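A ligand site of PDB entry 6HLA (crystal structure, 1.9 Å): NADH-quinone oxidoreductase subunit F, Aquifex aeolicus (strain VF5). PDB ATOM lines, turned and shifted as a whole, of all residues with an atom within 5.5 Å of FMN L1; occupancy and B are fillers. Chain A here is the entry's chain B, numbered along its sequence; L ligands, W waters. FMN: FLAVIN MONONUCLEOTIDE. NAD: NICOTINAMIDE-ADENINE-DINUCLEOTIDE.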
ATOM      1  N   GLY A  65      18.098  19.678  -5.232  1.00  0.00           N
ATOM      2  CA  GLY A  65      17.411  20.252  -4.083  1.00  0.00           C
ATOM      3  C   GLY A  65      17.693  19.528  -2.791  1.00  0.00           C
ATOM      4  O   GLY A  65      17.570  18.302  -2.722  1.00  0.00           O
ATOM      5  N   ARG A  66      18.083  20.288  -1.777  1.00  0.00           N
ATOM      6  CA  ARG A  66      18.479  19.794  -0.464  1.00  0.00           C
ATOM      7  C   ARG A  66      17.319  19.763   0.523  1.00  0.00           C
ATOM      8  O   ARG A  66      17.482  19.304   1.656  1.00  0.00           O
ATOM      9  CB  ARG A  66      19.695  20.589   0.071  1.00  0.00           C
ATOM     10  CG  ARG A  66      20.993  20.525  -0.752  1.00  0.00           C
ATOM     11  CD  ARG A  66      21.462  19.138  -1.066  1.00  0.00           C
ATOM     12  NE  ARG A  66      22.908  19.124  -1.293  1.00  0.00           N
ATOM     13  CZ  ARG A  66      23.484  18.721  -2.419  1.00  0.00           C
ATOM     14  NH1 ARG A  66      24.809  18.757  -2.558  1.00  0.00           N
ATOM     15  NH2 ARG A  66      22.741  18.239  -3.424  1.00  0.00           N
ATOM     16  N   GLY A  67      16.162  20.212   0.065  1.00  0.00           N
ATOM     17  CA  GLY A  67      14.942  20.238   0.854  1.00  0.00           C
ATOM     18  C   GLY A  67      14.361  18.861   1.098  1.00  0.00           C
ATOM     19  O   GLY A  67      13.537  18.702   1.992  1.00  0.00           O
ATOM     20  N   GLY A  68      14.757  17.879   0.294  1.00  0.00           N
ATOM     21  CA  GLY A  68      14.265  16.516   0.455  1.00  0.00           C
ATOM     22  C   GLY A  68      13.908  15.781  -0.819  1.00  0.00           C
ATOM     23  O   GLY A  68      14.038  14.565  -0.863  1.00  0.00           O
ATOM     24  N   ALA A  69      13.449  16.508  -1.860  1.00  0.00           N
ATOM     25  CA  ALA A  69      13.019  15.897  -3.126  1.00  0.00           C
ATOM     26  C   ALA A  69      14.120  15.742  -4.174  1.00  0.00           C
ATOM     27  O   ALA A  69      13.942  14.985  -5.114  1.00  0.00           O
ATOM     28  CB  ALA A  69      11.841  16.655  -3.701  1.00  0.00           C
ATOM     29  N   GLY A  70      15.234  16.461  -4.012  1.00  0.00           N
ATOM     30  CA  GLY A  70      16.359  16.377  -4.923  1.00  0.00           C
ATOM     31  C   GLY A  70      16.155  16.810  -6.354  1.00  0.00           C
ATOM     32  O   GLY A  70      16.793  16.228  -7.252  1.00  0.00           O
ATOM     33  N   PHE A  71      15.298  17.825  -6.590  1.00  0.00           N
ATOM     34  CA  PHE A  71      15.105  18.331  -7.956  1.00  0.00           C
ATOM     35  C   PHE A  71      16.352  19.094  -8.428  1.00  0.00           C
ATOM     36  O   PHE A  71      16.892  19.863  -7.643  1.00  0.00           O
ATOM     37  CB  PHE A  71      13.853  19.221  -8.081  1.00  0.00           C
ATOM     38  CG  PHE A  71      13.425  19.432  -9.527  1.00  0.00           C
ATOM     39  CD1 PHE A  71      13.820  20.569 -10.233  1.00  0.00           C
ATOM     40  CD2 PHE A  71      12.626  18.499 -10.172  1.00  0.00           C
ATOM     41  CE1 PHE A  71      13.472  20.752 -11.561  1.00  0.00           C
ATOM     42  CE2 PHE A  71      12.269  18.680 -11.515  1.00  0.00           C
ATOM     43  CZ  PHE A  71      12.700  19.798 -12.207  1.00  0.00           C
ATOM     44  N   THR A  73      18.624  21.846  -9.369  1.00  0.00           N
ATOM     45  CA  THR A  73      18.515  23.282  -9.106  1.00  0.00           C
ATOM     46  C   THR A  73      18.625  24.126 -10.374  1.00  0.00           C
ATOM     47  O   THR A  73      17.764  24.980 -10.578  1.00  0.00           O
ATOM     48  CB  THR A  73      19.507  23.690  -8.031  1.00  0.00           C
ATOM     49  OG1 THR A  73      19.350  22.765  -6.954  1.00  0.00           O
ATOM     50  CG2 THR A  73      19.281  25.104  -7.516  1.00  0.00           C
ATOM     51  N   LYS A  76      15.506  23.766 -12.357  1.00  0.00           N
ATOM     52  CA  LYS A  76      14.409  24.553 -11.803  1.00  0.00           C
ATOM     53  C   LYS A  76      14.475  26.002 -12.266  1.00  0.00           C
ATOM     54  O   LYS A  76      13.445  26.553 -12.638  1.00  0.00           O
ATOM     55  CB  LYS A  76      14.441  24.526 -10.276  1.00  0.00           C
ATOM     56  CG  LYS A  76      13.155  25.128  -9.671  1.00  0.00           C
ATOM     57  CD  LYS A  76      13.174  25.179  -8.158  1.00  0.00           C
ATOM     58  CE  LYS A  76      12.906  23.808  -7.631  1.00  0.00           C
ATOM     59  NZ  LYS A  76      12.954  23.791  -6.173  1.00  0.00           N
ATOM     60  N   ASN A  92      13.417  28.669   1.359  1.00  0.00           N
ATOM     61  CA  ASN A  92      12.553  27.906   2.261  1.00  0.00           C
ATOM     62  C   ASN A  92      13.287  27.546   3.566  1.00  0.00           C
ATOM     63  O   ASN A  92      14.105  26.635   3.574  1.00  0.00           O
ATOM     64  CB  ASN A  92      12.022  26.648   1.559  1.00  0.00           C
ATOM     65  CG  ASN A  92      10.908  25.966   2.293  1.00  0.00           C
ATOM     66  OD1 ASN A  92      10.711  26.143   3.510  1.00  0.00           O
ATOM     67  ND2 ASN A  92      10.163  25.163   1.552  1.00  0.00           N
ATOM     68  N   ALA A  93      12.967  28.245   4.673  1.00  0.00           N
ATOM     69  CA  ALA A  93      13.584  27.959   5.969  1.00  0.00           C
ATOM     70  C   ALA A  93      12.539  27.437   6.947  1.00  0.00           C
ATOM     71  O   ALA A  93      12.684  27.608   8.148  1.00  0.00           O
ATOM     72  CB  ALA A  93      14.285  29.204   6.519  1.00  0.00           C
ATOM     73  N   ASP A  94      11.518  26.727   6.416  1.00  0.00           N
ATOM     74  CA  ASP A  94      10.456  26.211   7.251  1.00  0.00           C
ATOM     75  C   ASP A  94      10.840  24.977   8.067  1.00  0.00           C
ATOM     76  O   ASP A  94      10.155  24.714   9.053  1.00  0.00           O
ATOM     77  CB  ASP A  94       9.137  25.961   6.474  1.00  0.00           C
ATOM     78  CG  ASP A  94       7.961  25.891   7.421  1.00  0.00           C
ATOM     79  OD1 ASP A  94       7.652  26.922   8.073  1.00  0.00           O
ATOM     80  OD2 ASP A  94       7.483  24.749   7.678  1.00  0.00           O
ATOM     81  N   GLU A  95      11.912  24.271   7.690  1.00  0.00           N
ATOM     82  CA  GLU A  95      12.455  23.038   8.312  1.00  0.00           C
ATOM     83  C   GLU A  95      11.614  22.509   9.463  1.00  0.00           C
ATOM     84  O   GLU A  95      11.784  22.947  10.610  1.00  0.00           O
ATOM     85  CB  GLU A  95      13.913  23.272   8.756  1.00  0.00           C
ATOM     86  CG  GLU A  95      14.560  22.035   9.314  1.00  0.00           C
ATOM     87  CD  GLU A  95      16.043  22.196   9.466  1.00  0.00           C
ATOM     88  OE1 GLU A  95      16.459  23.050  10.271  1.00  0.00           O
ATOM     89  OE2 GLU A  95      16.799  21.521   8.725  1.00  0.00           O
ATOM     90  N   SER A  96      10.629  21.636   9.152  1.00  0.00           N
ATOM     91  CA  SER A  96       9.743  21.123  10.195  1.00  0.00           C
ATOM     92  C   SER A  96       9.595  19.603  10.194  1.00  0.00           C
ATOM     93  O   SER A  96       8.832  19.055  10.993  1.00  0.00           O
ATOM     94  CB  SER A  96       8.390  21.821  10.105  1.00  0.00           C
ATOM     95  OG  SER A  96       8.501  23.164  10.547  1.00  0.00           O
ATOM     96  N   GLU A  97      10.360  18.912   9.323  1.00  0.00           N
ATOM     97  CA  GLU A  97      10.376  17.468   9.244  1.00  0.00           C
ATOM     98  C   GLU A  97      10.953  16.850  10.522  1.00  0.00           C
ATOM     99  O   GLU A  97      12.029  17.266  10.933  1.00  0.00           O
ATOM    100  CB  GLU A  97      11.206  17.029   8.028  1.00  0.00           C
ATOM    101  CG  GLU A  97      11.214  15.526   7.728  1.00  0.00           C
ATOM    102  CD  GLU A  97       9.911  14.920   7.249  1.00  0.00           C
ATOM    103  OE1 GLU A  97       9.921  13.729   6.891  1.00  0.00           O
ATOM    104  OE2 GLU A  97       8.884  15.640   7.195  1.00  0.00           O
ATOM    105  N   ASP A 103      19.332  22.817   8.451  1.00  0.00           N
ATOM    106  CA  ASP A 103      19.203  24.190   7.964  1.00  0.00           C
ATOM    107  C   ASP A 103      19.435  25.240   8.997  1.00  0.00           C
ATOM    108  O   ASP A 103      20.138  26.210   8.733  1.00  0.00           O
ATOM    109  CB  ASP A 103      17.825  24.439   7.330  1.00  0.00           C
ATOM    110  CG  ASP A 103      17.554  23.645   6.108  1.00  0.00           C
ATOM    111  OD1 ASP A 103      18.495  22.996   5.613  1.00  0.00           O
ATOM    112  OD2 ASP A 103      16.391  23.613   5.668  1.00  0.00           O
ATOM    113  N   TYR A 180       3.388  22.767   9.741  1.00  0.00           N
ATOM    114  CA  TYR A 180       4.391  21.978   9.007  1.00  0.00           C
ATOM    115  C   TYR A 180       4.163  22.082   7.494  1.00  0.00           C
ATOM    116  O   TYR A 180       5.116  22.153   6.730  1.00  0.00           O
ATOM    117  CB  TYR A 180       4.338  20.518   9.470  1.00  0.00           C
ATOM    118  CG  TYR A 180       4.906  19.476   8.538  1.00  0.00           C
ATOM    119  CD1 TYR A 180       6.283  19.255   8.475  1.00  0.00           C
ATOM    120  CD2 TYR A 180       4.071  18.650   7.808  1.00  0.00           C
ATOM    121  CE1 TYR A 180       6.804  18.246   7.671  1.00  0.00           C
ATOM    122  CE2 TYR A 180       4.583  17.638   7.003  1.00  0.00           C
ATOM    123  CZ  TYR A 180       5.944  17.435   6.934  1.00  0.00           C
ATOM    124  OH  TYR A 180       6.417  16.401   6.159  1.00  0.00           O
ATOM    125  N   ILE A 181       2.898  22.154   7.093  1.00  0.00           N
ATOM    126  CA  ILE A 181       2.450  22.272   5.714  1.00  0.00           C
ATOM    127  C   ILE A 181       2.952  23.533   5.015  1.00  0.00           C
ATOM    128  O   ILE A 181       3.033  23.557   3.797  1.00  0.00           O
ATOM    129  CB  ILE A 181       0.899  22.135   5.623  1.00  0.00           C
ATOM    130  CG1 ILE A 181       0.441  21.766   4.211  1.00  0.00           C
ATOM    131  CG2 ILE A 181       0.156  23.377   6.149  1.00  0.00           C
ATOM    132  CD1 ILE A 181       0.967  20.503   3.701  1.00  0.00           C
ATOM    133  N   GLY A 183       5.798  24.583   4.811  1.00  0.00           N
ATOM    134  CA  GLY A 183       7.102  24.323   4.210  1.00  0.00           C
ATOM    135  C   GLY A 183       6.897  23.790   2.807  1.00  0.00           C
ATOM    136  O   GLY A 183       7.818  23.848   1.989  1.00  0.00           O
ATOM    137  N   GLU A 184       5.653  23.226   2.516  1.00  0.00           N
ATOM    138  CA  GLU A 184       5.236  22.796   1.194  1.00  0.00           C
ATOM    139  C   GLU A 184       5.253  24.112   0.433  1.00  0.00           C
ATOM    140  O   GLU A 184       4.707  25.117   0.914  1.00  0.00           O
ATOM    141  CB  GLU A 184       3.831  22.151   1.237  1.00  0.00           C
ATOM    142  CG  GLU A 184       3.540  21.291   0.020  1.00  0.00           C
ATOM    143  CD  GLU A 184       3.078  22.026  -1.214  1.00  0.00           C
ATOM    144  OE1 GLU A 184       2.698  23.213  -1.107  1.00  0.00           O
ATOM    145  OE2 GLU A 184       3.078  21.400  -2.310  1.00  0.00           O
ATOM    146  N   GLU A 185       5.970  24.149  -0.668  1.00  0.00           N
ATOM    147  CA  GLU A 185       6.298  25.399  -1.382  1.00  0.00           C
ATOM    148  C   GLU A 185       5.105  26.223  -1.830  1.00  0.00           C
ATOM    149  O   GLU A 185       5.253  27.435  -1.892  1.00  0.00           O
ATOM    150  CB  GLU A 185       7.232  25.146  -2.547  1.00  0.00           C
ATOM    151  CG  GLU A 185       6.548  24.300  -3.602  1.00  0.00           C
ATOM    152  CD  GLU A 185       7.341  24.014  -4.833  1.00  0.00           C
ATOM    153  OE1 GLU A 185       8.486  24.513  -4.963  1.00  0.00           O
ATOM    154  OE2 GLU A 185       6.784  23.298  -5.706  1.00  0.00           O
ATOM    155  N   VAL A 218      11.498  28.448  -5.529  1.00  0.00           N
ATOM    156  CA  VAL A 218      11.559  28.133  -4.096  1.00  0.00           C
ATOM    157  C   VAL A 218      12.700  27.151  -3.940  1.00  0.00           C
ATOM    158  O   VAL A 218      12.706  26.118  -4.610  1.00  0.00           O
ATOM    159  CB  VAL A 218      10.238  27.559  -3.509  1.00  0.00           C
ATOM    160  CG1 VAL A 218      10.374  27.285  -2.015  1.00  0.00           C
ATOM    161  CG2 VAL A 218       9.055  28.485  -3.781  1.00  0.00           C
ATOM    162  N   ASN A 219      13.696  27.498  -3.108  1.00  0.00           N
ATOM    163  CA  ASN A 219      14.816  26.604  -2.830  1.00  0.00           C
ATOM    164  C   ASN A 219      15.062  26.517  -1.350  1.00  0.00           C
ATOM    165  O   ASN A 219      14.844  27.477  -0.648  1.00  0.00           O
ATOM    166  CB  ASN A 219      16.089  27.016  -3.560  1.00  0.00           C
ATOM    167  CG  ASN A 219      16.208  26.494  -4.971  1.00  0.00           C
ATOM    168  OD1 ASN A 219      16.363  27.273  -5.907  1.00  0.00           O
ATOM    169  ND2 ASN A 219      16.195  25.175  -5.145  1.00  0.00           N
ATOM    170  N   ASN A 220      15.480  25.368  -0.879  1.00  0.00           N
ATOM    171  CA  ASN A 220      15.785  25.098   0.515  1.00  0.00           C
ATOM    172  C   ASN A 220      17.066  25.866   0.924  1.00  0.00           C
ATOM    173  O   ASN A 220      17.904  26.159   0.089  1.00  0.00           O
ATOM    174  CB  ASN A 220      16.003  23.596   0.674  1.00  0.00           C
ATOM    175  CG  ASN A 220      16.505  23.156   2.023  1.00  0.00           C
ATOM    176  OD1 ASN A 220      17.687  22.924   2.214  1.00  0.00           O
ATOM    177  ND2 ASN A 220      15.643  23.119   3.005  1.00  0.00           N
ATOM    178  N   VAL A 221      17.197  26.174   2.225  1.00  0.00           N
ATOM    179  CA  VAL A 221      18.373  26.831   2.842  1.00  0.00           C
ATOM    180  C   VAL A 221      19.668  26.144   2.400  1.00  0.00           C
ATOM    181  O   VAL A 221      20.594  26.795   1.911  1.00  0.00           O
ATOM    182  CB  VAL A 221      18.228  26.816   4.413  1.00  0.00           C
ATOM    183  CG1 VAL A 221      19.527  27.222   5.112  1.00  0.00           C
ATOM    184  CG2 VAL A 221      17.097  27.714   4.856  1.00  0.00           C
ATOM    185  N   THR A 223      20.315  24.072  -0.116  1.00  0.00           N
ATOM    186  CA  THR A 223      20.537  24.169  -1.565  1.00  0.00           C
ATOM    187  C   THR A 223      21.213  25.528  -1.853  1.00  0.00           C
ATOM    188  O   THR A 223      22.228  25.576  -2.537  1.00  0.00           O
ATOM    189  CB  THR A 223      19.214  24.088  -2.316  1.00  0.00           C
ATOM    190  OG1 THR A 223      18.480  22.951  -1.880  1.00  0.00           O
ATOM    191  CG2 THR A 223      19.411  24.017  -3.828  1.00  0.00           C
ATOM    192  N   CYS A 393      -0.831  17.569  -2.498  1.00  0.00           N
ATOM    193  CA  CYS A 393       0.543  17.824  -2.024  1.00  0.00           C
ATOM    194  C   CYS A 393       1.173  16.545  -1.478  1.00  0.00           C
ATOM    195  O   CYS A 393       0.486  15.529  -1.317  1.00  0.00           O
ATOM    196  CB  CYS A 393       0.634  19.005  -1.051  1.00  0.00           C
ATOM    197  SG  CYS A 393       0.580  18.601   0.713  1.00  0.00           S
ATOM    198  N   GLY A 394       2.490  16.580  -1.275  1.00  0.00           N
ATOM    199  CA  GLY A 394       3.265  15.417  -0.834  1.00  0.00           C
ATOM    200  C   GLY A 394       2.893  14.831   0.520  1.00  0.00           C
ATOM    201  O   GLY A 394       3.197  13.664   0.752  1.00  0.00           O
ATOM    202  N   LEU A 395       2.264  15.617   1.419  1.00  0.00           N
ATOM    203  CA  LEU A 395       1.857  15.176   2.766  1.00  0.00           C
ATOM    204  C   LEU A 395       0.871  13.982   2.719  1.00  0.00           C
ATOM    205  O   LEU A 395       1.117  12.969   3.391  1.00  0.00           O
ATOM    206  CB  LEU A 395       1.298  16.355   3.621  1.00  0.00           C
ATOM    207  CG  LEU A 395       1.158  16.078   5.135  1.00  0.00           C
ATOM    208  CD1 LEU A 395       1.200  17.349   5.913  1.00  0.00           C
ATOM    209  CD2 LEU A 395      -0.180  15.319   5.464  1.00  0.00           C
HETATM  210  N1  FMN L   1      11.267  21.944   1.716  1.00  0.00           N
HETATM  211  C2  FMN L   1      12.067  22.723   2.508  1.00  0.00           C
HETATM  212  O2  FMN L   1      13.056  23.296   2.052  1.00  0.00           O
HETATM  213  N3  FMN L   1      11.713  22.951   3.839  1.00  0.00           N
HETATM  214  C4  FMN L   1      10.562  22.490   4.466  1.00  0.00           C
HETATM  215  O4  FMN L   1      10.360  22.758   5.650  1.00  0.00           O
HETATM  216  C4A FMN L   1       9.692  21.694   3.595  1.00  0.00           C
HETATM  217  N5  FMN L   1       8.536  21.304   4.072  1.00  0.00           N
HETATM  218  C5A FMN L   1       7.675  20.607   3.219  1.00  0.00           C
HETATM  219  C6  FMN L   1       6.458  20.134   3.726  1.00  0.00           C
HETATM  220  C7  FMN L   1       5.616  19.347   2.950  1.00  0.00           C
HETATM  221  C7M FMN L   1       4.329  18.829   3.546  1.00  0.00           C
HETATM  222  C8  FMN L   1       5.981  19.047   1.626  1.00  0.00           C
HETATM  223  C8M FMN L   1       5.105  18.176   0.746  1.00  0.00           C
HETATM  224  C9  FMN L   1       7.172  19.542   1.106  1.00  0.00           C
HETATM  225  C9A FMN L   1       8.026  20.318   1.896  1.00  0.00           C
HETATM  226  N10 FMN L   1       9.285  20.787   1.407  1.00  0.00           N
HETATM  227  C10 FMN L   1      10.143  21.471   2.229  1.00  0.00           C
HETATM  228  C1' FMN L   1       9.630  20.653  -0.015  1.00  0.00           C
HETATM  229  C2' FMN L   1       9.256  21.890  -0.829  1.00  0.00           C
HETATM  230  O2' FMN L   1       7.879  21.813  -1.220  1.00  0.00           O
HETATM  231  C3' FMN L   1      10.177  22.055  -2.036  1.00  0.00           C
HETATM  232  O3' FMN L   1      10.391  20.789  -2.671  1.00  0.00           O
HETATM  233  C4' FMN L   1      11.553  22.670  -1.750  1.00  0.00           C
HETATM  234  O4' FMN L   1      11.491  23.743  -0.802  1.00  0.00           O
HETATM  235  C5' FMN L   1      12.232  23.119  -3.016  1.00  0.00           C
HETATM  236  O5' FMN L   1      13.611  23.420  -2.707  1.00  0.00           O
HETATM  237  P   FMN L   1      14.815  22.505  -3.110  1.00  0.00           P
HETATM  238  O1P FMN L   1      14.851  21.298  -2.283  1.00  0.00           O
HETATM  239  O2P FMN L   1      14.597  22.139  -4.595  1.00  0.00           O
HETATM  240  O3P FMN L   1      16.080  23.388  -2.968  1.00  0.00           O
HETATM  241  PA  NAD L   2       8.624  17.399  -5.699  1.00  0.00           P
HETATM  242  O1A NAD L   2       9.419  16.207  -6.087  1.00  0.00           O
HETATM  243  O2A NAD L   2       7.270  17.353  -6.370  1.00  0.00           O
HETATM  244  O5B NAD L   2       9.352  18.760  -6.247  1.00  0.00           O
HETATM  245  C5B NAD L   2      10.630  19.264  -5.817  1.00  0.00           C
HETATM  246  C4B NAD L   2      10.831  20.634  -6.407  1.00  0.00           C
HETATM  247  O4B NAD L   2      10.972  20.515  -7.836  1.00  0.00           O
HETATM  248  C3B NAD L   2       9.750  21.685  -6.172  1.00  0.00           C
HETATM  249  O3B NAD L   2      10.350  22.969  -6.046  1.00  0.00           O
HETATM  250  C2B NAD L   2       8.929  21.619  -7.466  1.00  0.00           C
HETATM  251  O2B NAD L   2       8.227  22.813  -7.798  1.00  0.00           O
HETATM  252  C1B NAD L   2      10.019  21.354  -8.484  1.00  0.00           C
HETATM  253  N9A NAD L   2       9.543  20.662  -9.676  1.00  0.00           N
HETATM  254  C8A NAD L   2       9.171  19.344  -9.759  1.00  0.00           C
HETATM  255  N7A NAD L   2       8.724  18.990 -10.940  1.00  0.00           N
HETATM  256  C5A NAD L   2       8.806  20.161 -11.682  1.00  0.00           C
HETATM  257  C6A NAD L   2       8.440  20.465 -13.006  1.00  0.00           C
HETATM  258  N6A NAD L   2       7.798  19.626 -13.814  1.00  0.00           N
HETATM  259  N1A NAD L   2       8.669  21.727 -13.448  1.00  0.00           N
HETATM  260  C2A NAD L   2       9.194  22.621 -12.608  1.00  0.00           C
HETATM  261  N3A NAD L   2       9.541  22.456 -11.320  1.00  0.00           N
HETATM  262  C4A NAD L   2       9.316  21.199 -10.920  1.00  0.00           C
HETATM  263  O3  NAD L   2       8.394  17.378  -4.114  1.00  0.00           O
HETATM  264  PN  NAD L   2       7.723  18.272  -2.971  1.00  0.00           P
HETATM  265  O1N NAD L   2       6.338  17.807  -2.770  1.00  0.00           O
HETATM  266  O2N NAD L   2       7.954  19.700  -3.252  1.00  0.00           O
HETATM  267  O5D NAD L   2       8.623  17.844  -1.725  1.00  0.00           O
HETATM  268  C5D NAD L   2       8.622  16.520  -1.164  1.00  0.00           C
HETATM  269  C4D NAD L   2       9.807  16.435  -0.215  1.00  0.00           C
HETATM  270  O4D NAD L   2       9.679  17.410   0.839  1.00  0.00           O
HETATM  271  C3D NAD L   2       9.993  15.091   0.509  1.00  0.00           C
HETATM  272  O3D NAD L   2      10.908  14.205  -0.114  1.00  0.00           O
HETATM  273  C2D NAD L   2      10.464  15.487   1.918  1.00  0.00           C
HETATM  274  O2D NAD L   2      11.753  14.993   2.275  1.00  0.00           O
HETATM  275  C1D NAD L   2      10.567  17.014   1.830  1.00  0.00           C
HETATM  276  N1N NAD L   2      10.181  17.710   3.153  1.00  0.00           N
HETATM  277  C2N NAD L   2      11.200  18.378   3.730  1.00  0.00           C
HETATM  278  C3N NAD L   2      11.042  18.946   4.986  1.00  0.00           C
HETATM  279  C7N NAD L   2      12.183  19.662   5.649  1.00  0.00           C
HETATM  280  O7N NAD L   2      12.065  20.032   6.837  1.00  0.00           O
HETATM  281  N7N NAD L   2      13.332  19.783   4.971  1.00  0.00           N
HETATM  282  C4N NAD L   2       9.804  18.831   5.601  1.00  0.00           C
HETATM  283  C5N NAD L   2       8.767  18.130   4.991  1.00  0.00           C
HETATM  284  C6N NAD L   2       8.981  17.579   3.755  1.00  0.00           C
HETATM  285  O   HOH W   1       7.810  22.150   7.004  1.00  0.00           O
HETATM  286  O   HOH W   2      13.901  19.521  -4.861  1.00  0.00           O
HETATM  287  O   HOH W   3      13.904  24.511   5.151  1.00  0.00           O
HETATM  288  O   HOH W   4      12.903  19.289  -1.991  1.00  0.00           O
HETATM  289  O   HOH W   5      16.458  22.347  -6.549  1.00  0.00           O
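An oxygen (O7N) of NAD L2 sits at hydrogen-bond distance from the backbone NH of Ser 96 (3.2 Å).
An oxygen (O2P) of FMN L1 lies within salt-bridge range of the side-chain amino group of Lys 76 (2.8 Å).
O3P of FMN L1 lies within hydrogen-bond range of N of Asn 220, 2.9 Å away.
The backbone carbonyl oxygen (O) of Gly 68 sits at hydrogen-bond distance from an oxygen (O3D) of NAD L2, at 3.2 Å.
The backbone NH of Arg 66 is in hydrogen-bond range of an oxygen (O1P) of FMN L1.
The backbone NH of Gly 67 is in hydrogen-bond range of an oxygen (O1P) of FMN L1 (2.9 Å).
The backbone NH of Glu 185 lies within hydrogen-bond range of an oxygen (O2') of FMN L1, at 3.1 Å.
NZ of Lys 76 sits at hydrogen-bond distance from O3B of NAD L2 (2.7 Å).
OE2 of Glu 185 is in hydrogen-bond range of O2B of NAD L2.
OG1 of Thr 223 is in hydrogen-bond range of O3P of FMN L1.
The backbone NH of Glu 95 is in hydrogen-bond range of an oxygen (O4) of FMN L1, 3.0 Å away.
ND2 of Asn 92 sits at hydrogen-bond distance from O4' of FMN L1 (3.1 Å).
The backbone NH (N) of Glu 97 sits at hydrogen-bond distance from an oxygen (O7N) of NAD L2, at 3.2 Å.
ND2 of Asn 220 lies within hydrogen-bond range of O2 of FMN L1 (2.8 Å).
O3P of FMN L1 lies within hydrogen-bond range of ND2 of Asn 219 (2.8 Å).
N7N of NAD L2 sits close to O of Gly 67, at 3.2 Å.
O3' of FMN L1 sits at hydrogen-bond distance from O2N of NAD L2 (2.7 Å).
The side-chain carboxylate (OD2) of Asp 103 is in hydrogen-bond range of the side-chain amide nitrogen (ND2) of Asn 220 (2.8 Å).
The backbone NH (N) of Gly 70 lies close to the backbone carbonyl oxygen (O) of Gly 65.
The backbone NH (N) of Asn 92 lies within hydrogen-bond range of the backbone carbonyl oxygen (O) of Asn 219.
OG1 of Thr 223 lies within hydrogen-bond range of N of Arg 66, 2.7 Å away.
The backbone carbonyl oxygen of Val 218 is in hydrogen-bond range of the side-chain amino group of Lys 76, 2.8 Å away.
The backbone carbonyl oxygen of Gly 183 is in hydrogen-bond range of the side-chain amide nitrogen of Asn 92.
OE2 of Glu 97 lies within hydrogen-bond range of OH of Tyr 180 (2.8 Å).
The side-chain carboxylate (OD2) of Asp 94 lies within hydrogen-bond range of the backbone NH (N) of Gly 183.
A nitrogen (N5) of FMN L1 sits close to the backbone carbonyl oxygen (O) of Gly 183 (3.4 Å).
O5' of FMN L1 sits close to O of Val 218 (3.4 Å).
Merely in contact with FMN L1: Gly 65 (3.3 Å), Asp 94 (3.3 Å), Glu 184 (3.4 Å), Tyr 180 (3.7 Å), Gly 394 (3.7 Å), Ser 96 (3.7 Å), Ile 181 (3.8 Å) and Leu 395 (3.9 Å).
The nearest printed residue that does not touch FMN L1 is Gly 68 (4.3 Å).
Water W5 lies within hydrogen-bond range of O2P of FMN L1, O of Phe 71, OG1 of Thr 73, ND2 of Asn 219 and N of Gly 65.
Water W2 lies within hydrogen-bond range of an oxygen (O2P) of FMN L1 (2.7 Å), the backbone NH (N) of Phe 71 (2.8 Å) and the backbone NH (N) of Gly 70 (3.4 Å).
Water W4 lies within hydrogen-bond range of O1P of FMN L1 (2.8 Å), N of Ala 69 (2.8 Å) and N of Gly 68 (3.3 Å).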
